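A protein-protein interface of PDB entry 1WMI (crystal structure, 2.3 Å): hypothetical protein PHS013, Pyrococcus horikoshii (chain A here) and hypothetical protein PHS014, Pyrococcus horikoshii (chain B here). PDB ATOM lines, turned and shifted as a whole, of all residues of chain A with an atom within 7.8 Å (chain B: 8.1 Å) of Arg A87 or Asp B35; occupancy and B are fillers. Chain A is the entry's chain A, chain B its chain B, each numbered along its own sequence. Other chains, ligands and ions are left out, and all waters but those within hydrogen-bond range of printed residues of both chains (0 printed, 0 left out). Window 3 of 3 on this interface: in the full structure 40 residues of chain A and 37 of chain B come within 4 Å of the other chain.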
ATOM      1  N   ARG A  60      -0.317   9.177 -20.337  1.00  0.00           N
ATOM      2  CA  ARG A  60       0.097  10.547 -20.566  1.00  0.00           C
ATOM      3  C   ARG A  60      -0.062  11.333 -19.258  1.00  0.00           C
ATOM      4  O   ARG A  60      -1.160  11.421 -18.691  1.00  0.00           O
ATOM      5  CB  ARG A  60      -0.744  11.158 -21.699  1.00  0.00           C
ATOM      6  CG  ARG A  60      -0.251  12.510 -22.194  1.00  0.00           C
ATOM      7  CD  ARG A  60      -1.024  12.977 -23.422  1.00  0.00           C
ATOM      8  NE  ARG A  60      -0.701  12.197 -24.616  1.00  0.00           N
ATOM      9  CZ  ARG A  60       0.488  12.193 -25.216  1.00  0.00           C
ATOM     10  NH1 ARG A  60       0.682  11.452 -26.300  1.00  0.00           N
ATOM     11  NH2 ARG A  60       1.486  12.930 -24.739  1.00  0.00           N
ATOM     12  N   ARG A  65       5.261  11.134 -21.231  1.00  0.00           N
ATOM     13  CA  ARG A  65       4.496   9.893 -21.287  1.00  0.00           C
ATOM     14  C   ARG A  65       5.224   8.760 -20.570  1.00  0.00           C
ATOM     15  O   ARG A  65       6.458   8.700 -20.572  1.00  0.00           O
ATOM     16  CB  ARG A  65       4.262   9.494 -22.745  1.00  0.00           C
ATOM     17  CG  ARG A  65       3.372  10.450 -23.528  1.00  0.00           C
ATOM     18  CD  ARG A  65       3.429  10.141 -25.014  1.00  0.00           C
ATOM     19  NE  ARG A  65       4.740  10.466 -25.567  1.00  0.00           N
ATOM     20  CZ  ARG A  65       5.232   9.949 -26.688  1.00  0.00           C
ATOM     21  NH1 ARG A  65       6.437  10.312 -27.112  1.00  0.00           N
ATOM     22  NH2 ARG A  65       4.528   9.060 -27.376  1.00  0.00           N
ATOM     23  N   ILE A  67       5.408   4.503 -20.127  1.00  0.00           N
ATOM     24  CA  ILE A  67       5.019   3.204 -20.664  1.00  0.00           C
ATOM     25  C   ILE A  67       5.215   2.157 -19.573  1.00  0.00           C
ATOM     26  O   ILE A  67       6.259   2.111 -18.922  1.00  0.00           O
ATOM     27  CB  ILE A  67       5.854   2.821 -21.902  1.00  0.00           C
ATOM     28  CG1 ILE A  67       5.657   3.864 -23.001  1.00  0.00           C
ATOM     29  CG2 ILE A  67       5.415   1.460 -22.422  1.00  0.00           C
ATOM     30  CD1 ILE A  67       6.269   3.469 -24.349  1.00  0.00           C
ATOM     31  N   LYS A  81       9.402   2.795 -18.996  1.00  0.00           N
ATOM     32  CA  LYS A  81      10.180   3.966 -19.389  1.00  0.00           C
ATOM     33  C   LYS A  81       9.359   5.233 -19.585  1.00  0.00           C
ATOM     34  O   LYS A  81       8.129   5.205 -19.571  1.00  0.00           O
ATOM     35  CB  LYS A  81      10.961   3.682 -20.676  1.00  0.00           C
ATOM     36  CG  LYS A  81      10.090   3.586 -21.913  1.00  0.00           C
ATOM     37  CD  LYS A  81      10.921   3.553 -23.178  1.00  0.00           C
ATOM     38  CE  LYS A  81      11.699   4.845 -23.374  1.00  0.00           C
ATOM     39  NZ  LYS A  81      12.441   4.824 -24.674  1.00  0.00           N
ATOM     40  N   LYS A  83       8.868   9.020 -21.863  1.00  0.00           N
ATOM     41  CA  LYS A  83       9.009   9.586 -23.198  1.00  0.00           C
ATOM     42  C   LYS A  83       8.557  11.051 -23.217  1.00  0.00           C
ATOM     43  O   LYS A  83       7.757  11.479 -22.376  1.00  0.00           O
ATOM     44  CB  LYS A  83       8.201   8.771 -24.213  1.00  0.00           C
ATOM     45  CG  LYS A  83       8.742   7.364 -24.447  1.00  0.00           C
ATOM     46  CD  LYS A  83       7.880   6.607 -25.448  1.00  0.00           C
ATOM     47  CE  LYS A  83       8.352   6.786 -26.890  1.00  0.00           C
ATOM     48  NZ  LYS A  83       9.498   5.892 -27.212  1.00  0.00           N
ATOM     49  N   PRO A  84       9.076  11.838 -24.177  1.00  0.00           N
ATOM     50  CA  PRO A  84       8.737  13.258 -24.317  1.00  0.00           C
ATOM     51  C   PRO A  84       7.243  13.470 -24.525  1.00  0.00           C
ATOM     52  O   PRO A  84       6.484  12.511 -24.621  1.00  0.00           O
ATOM     53  CB  PRO A  84       9.544  13.686 -25.542  1.00  0.00           C
ATOM     54  CG  PRO A  84      10.720  12.791 -25.501  1.00  0.00           C
ATOM     55  CD  PRO A  84      10.099  11.456 -25.165  1.00  0.00           C
ATOM     56  N   ARG A  85       6.840  14.734 -24.597  1.00  0.00           N
ATOM     57  CA  ARG A  85       5.447  15.124 -24.807  1.00  0.00           C
ATOM     58  C   ARG A  85       4.900  14.309 -25.970  1.00  0.00           C
ATOM     59  O   ARG A  85       3.732  13.891 -25.983  1.00  0.00           O
ATOM     60  CB  ARG A  85       5.380  16.601 -25.204  1.00  0.00           C
ATOM     61  CG  ARG A  85       4.205  17.371 -24.639  1.00  0.00           C
ATOM     62  CD  ARG A  85       4.515  17.824 -23.232  1.00  0.00           C
ATOM     63  NE  ARG A  85       4.775  19.260 -23.124  1.00  0.00           N
ATOM     64  CZ  ARG A  85       4.031  20.094 -22.404  1.00  0.00           C
ATOM     65  NH1 ARG A  85       2.984  19.634 -21.735  1.00  0.00           N
ATOM     66  NH2 ARG A  85       4.334  21.383 -22.348  1.00  0.00           N
ATOM     67  N   GLY A  86       5.795  14.088 -26.928  1.00  0.00           N
ATOM     68  CA  GLY A  86       5.495  13.390 -28.162  1.00  0.00           C
ATOM     69  C   GLY A  86       5.780  14.536 -29.098  1.00  0.00           C
ATOM     70  O   GLY A  86       4.958  15.453 -29.230  1.00  0.00           O
ATOM     71  N   ARG A  87       6.961  14.501 -29.707  1.00  0.00           N
ATOM     72  CA  ARG A  87       7.418  15.568 -30.587  1.00  0.00           C
ATOM     73  C   ARG A  87       6.470  16.076 -31.661  1.00  0.00           C
ATOM     74  O   ARG A  87       6.924  16.538 -32.693  1.00  0.00           O
ATOM     75  CB  ARG A  87       8.755  15.188 -31.232  1.00  0.00           C
ATOM     76  CG  ARG A  87       9.345  13.891 -30.718  1.00  0.00           C
ATOM     77  CD  ARG A  87      10.791  14.054 -30.245  1.00  0.00           C
ATOM     78  NE  ARG A  87      11.472  12.764 -30.126  1.00  0.00           N
ATOM     79  CZ  ARG A  87      12.694  12.590 -29.626  1.00  0.00           C
ATOM     80  NH1 ARG A  87      13.400  13.622 -29.180  1.00  0.00           N
ATOM     81  NH2 ARG A  87      13.213  11.369 -29.577  1.00  0.00           N
ATOM     82  N   ALA A  88       5.167  16.033 -31.391  1.00  0.00           N
ATOM     83  CA  ALA A  88       4.147  16.491 -32.323  1.00  0.00           C
ATOM     84  C   ALA A  88       2.741  16.316 -31.734  1.00  0.00           C
ATOM     85  O   ALA A  88       2.638  15.746 -30.627  1.00  0.00           O
ATOM     86  CB  ALA A  88       4.278  15.723 -33.637  1.00  0.00           C
ATOM     87  N   ARG B  32      -0.619   2.686 -30.927  1.00  0.00           N
ATOM     88  CA  ARG B  32       0.659   3.343 -30.679  1.00  0.00           C
ATOM     89  C   ARG B  32       0.632   4.836 -30.986  1.00  0.00           C
ATOM     90  O   ARG B  32      -0.405   5.402 -31.318  1.00  0.00           O
ATOM     91  CB  ARG B  32       1.757   2.711 -31.543  1.00  0.00           C
ATOM     92  CG  ARG B  32       2.244   1.337 -31.102  1.00  0.00           C
ATOM     93  CD  ARG B  32       1.226   0.244 -31.355  1.00  0.00           C
ATOM     94  NE  ARG B  32       1.825  -1.079 -31.202  1.00  0.00           N
ATOM     95  CZ  ARG B  32       1.150  -2.218 -31.295  1.00  0.00           C
ATOM     96  NH1 ARG B  32       1.775  -3.380 -31.144  1.00  0.00           N
ATOM     97  NH2 ARG B  32      -0.154  -2.190 -31.536  1.00  0.00           N
ATOM     98  N   ASP B  33       1.799   5.456 -30.842  1.00  0.00           N
ATOM     99  CA  ASP B  33       2.018   6.863 -31.154  1.00  0.00           C
ATOM    100  C   ASP B  33       3.166   6.744 -32.166  1.00  0.00           C
ATOM    101  O   ASP B  33       3.935   5.784 -32.088  1.00  0.00           O
ATOM    102  CB  ASP B  33       2.510   7.653 -29.928  1.00  0.00           C
ATOM    103  CG  ASP B  33       1.568   7.567 -28.737  1.00  0.00           C
ATOM    104  OD1 ASP B  33       0.340   7.685 -28.917  1.00  0.00           O
ATOM    105  OD2 ASP B  33       2.071   7.400 -27.606  1.00  0.00           O
ATOM    106  N   GLU B  34       3.286   7.674 -33.114  1.00  0.00           N
ATOM    107  CA  GLU B  34       4.378   7.596 -34.096  1.00  0.00           C
ATOM    108  C   GLU B  34       5.649   7.169 -33.383  1.00  0.00           C
ATOM    109  O   GLU B  34       6.324   6.211 -33.762  1.00  0.00           O
ATOM    110  CB  GLU B  34       4.643   8.957 -34.733  1.00  0.00           C
ATOM    111  CG  GLU B  34       3.595   9.433 -35.683  1.00  0.00           C
ATOM    112  CD  GLU B  34       4.102  10.569 -36.550  1.00  0.00           C
ATOM    113  OE1 GLU B  34       4.512  11.603 -35.986  1.00  0.00           O
ATOM    114  OE2 GLU B  34       4.099  10.429 -37.794  1.00  0.00           O
ATOM    115  N   ASP B  35       5.942   7.922 -32.334  1.00  0.00           N
ATOM    116  CA  ASP B  35       7.098   7.736 -31.478  1.00  0.00           C
ATOM    117  C   ASP B  35       7.423   6.293 -31.095  1.00  0.00           C
ATOM    118  O   ASP B  35       8.591   5.939 -30.926  1.00  0.00           O
ATOM    119  CB  ASP B  35       6.883   8.559 -30.207  1.00  0.00           C
ATOM    120  CG  ASP B  35       8.003   9.532 -29.952  1.00  0.00           C
ATOM    121  OD1 ASP B  35       7.769  10.545 -29.260  1.00  0.00           O
ATOM    122  OD2 ASP B  35       9.124   9.276 -30.442  1.00  0.00           O
ATOM    123  N   ILE B  36       6.396   5.461 -30.965  1.00  0.00           N
ATOM    124  CA  ILE B  36       6.587   4.073 -30.551  1.00  0.00           C
ATOM    125  C   ILE B  36       6.538   3.045 -31.679  1.00  0.00           C
ATOM    126  O   ILE B  36       5.549   2.944 -32.401  1.00  0.00           O
ATOM    127  CB  ILE B  36       5.560   3.720 -29.457  1.00  0.00           C
ATOM    128  CG1 ILE B  36       5.647   4.779 -28.355  1.00  0.00           C
ATOM    129  CG2 ILE B  36       5.846   2.338 -28.876  1.00  0.00           C
ATOM    130  CD1 ILE B  36       4.594   4.674 -27.280  1.00  0.00           C
ATOM    131  N   THR B  37       7.613   2.268 -31.795  1.00  0.00           N
ATOM    132  CA  THR B  37       7.763   1.249 -32.835  1.00  0.00           C
ATOM    133  C   THR B  37       7.509  -0.183 -32.346  1.00  0.00           C
ATOM    134  O   THR B  37       7.582  -0.462 -31.153  1.00  0.00           O
ATOM    135  CB  THR B  37       9.171   1.313 -33.419  1.00  0.00           C
ATOM    136  OG1 THR B  37       9.916   0.181 -32.967  1.00  0.00           O
ATOM    137  CG2 THR B  37       9.876   2.591 -32.957  1.00  0.00           C
ATOM    138  N   GLU B  38       7.224  -1.091 -33.276  1.00  0.00           N
ATOM    139  CA  GLU B  38       6.947  -2.484 -32.926  1.00  0.00           C
ATOM    140  C   GLU B  38       8.204  -3.000 -32.259  1.00  0.00           C
ATOM    141  O   GLU B  38       8.167  -3.820 -31.330  1.00  0.00           O
ATOM    142  CB  GLU B  38       6.644  -3.306 -34.179  1.00  0.00           C
ATOM    143  CG  GLU B  38       7.681  -3.202 -35.287  1.00  0.00           C
ATOM    144  CD  GLU B  38       8.402  -4.512 -35.538  1.00  0.00           C
ATOM    145  OE1 GLU B  38       7.712  -5.548 -35.645  1.00  0.00           O
ATOM    146  OE2 GLU B  38       9.650  -4.505 -35.642  1.00  0.00           O
ATOM    147  N   GLU B  40      10.631  -1.343 -30.401  1.00  0.00           N
ATOM    148  CA  GLU B  40      10.637  -0.863 -29.042  1.00  0.00           C
ATOM    149  C   GLU B  40       9.615  -1.589 -28.187  1.00  0.00           C
ATOM    150  O   GLU B  40       9.841  -1.799 -27.000  1.00  0.00           O
ATOM    151  CB  GLU B  40      10.382   0.639 -29.076  1.00  0.00           C
ATOM    152  CG  GLU B  40       9.977   1.273 -27.776  1.00  0.00           C
ATOM    153  CD  GLU B  40       9.792   2.772 -27.916  1.00  0.00           C
ATOM    154  OE1 GLU B  40       9.142   3.199 -28.894  1.00  0.00           O
ATOM    155  OE2 GLU B  40      10.285   3.526 -27.051  1.00  0.00           O
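OD2 of Asp B33 lies within salt-bridge range of NH2 of Arg A65 (3.0 Å). NH1 of Arg A65 is in salt-bridge range of OD1 of Asp B35 (2.5 Å). The side-chain carboxylate (OE2) of Glu B40 lies within salt-bridge range of the side-chain amino group (NZ) of Lys A81, 3.5 Å away. The side-chain carboxylate of Glu B40 lies within salt-bridge range of the side-chain amino group of Lys A83 (2.5 Å).
The backbone carbonyl oxygen (O) of Arg A65 is in hydrogen-bond range of the backbone NH (N) of Lys A83, at 2.8 Å. The guanidinium group (NE) of Arg A65 lies within hydrogen-bond range of the backbone carbonyl oxygen (O) of Pro A84, 2.8 Å away. The backbone NH (N) of Ile A67 sits at hydrogen-bond distance from the backbone carbonyl oxygen (O) of Lys A81. The side-chain hydroxyl (OG1) of Thr B37 is in hydrogen-bond range of the backbone NH (N) of Glu B40 (3.1 Å).
Ile B36 touches Ile A67. O of Asp B35 touches NZ of Lys A83, at 3.8 Å. CE of Lys A83 touches CG1 of Ile B36, at 3.7 Å. CA of Gly A86 touches OD1 of Asp B35 (3.8 Å). Asp B35 touches Arg A87.
Printed residues of chain B within 4 Å of Arg A65: Asp B33 (3.0 Å) and Asp B35 (2.5 Å). Of chain B, only Asp B35 (3.8 Å) comes within 4 Å of Gly A86. Of the printed residues of chain B, Arg A87 touches Asp B35 (3.98 Å). No residue of chain B comes within 4 Å of Ala A88. Arg B32 touches none of the printed residues of chain A. Of chain A, only Arg A65, Lys A83, Gly A86 and Arg A87 come within 4 Å of Asp B35. Printed residues of chain A within 4 Å of Ile B36: Ile A67 and Lys A83. Of the printed residues of chain A, Glu B40 touches Lys A81 (3.5 Å) and Lys A83 (2.5 Å). The nearest residue of chain A that does not touch Asp B35 is Pro A84 (4.8 Å). The nearest printed residue of chain A that does not touch Ile B36 is Arg A65 (4.4 Å).
Of the 8 printed residues of chain B, 4 touch a printed residue of chain A. Printed residues of chain B that touch a printed residue of chain A: Asp B33, Asp B35, Ile B36 and Glu B40. Hydrophobic or aromatic side chains of chain A within 4 Å of the printed part of chain B: Ile A67. Along chain A the printed residues that touch a printed residue of chain B span positions 65 to 87. Among the printed residues, 9 pairs touch across the chains.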
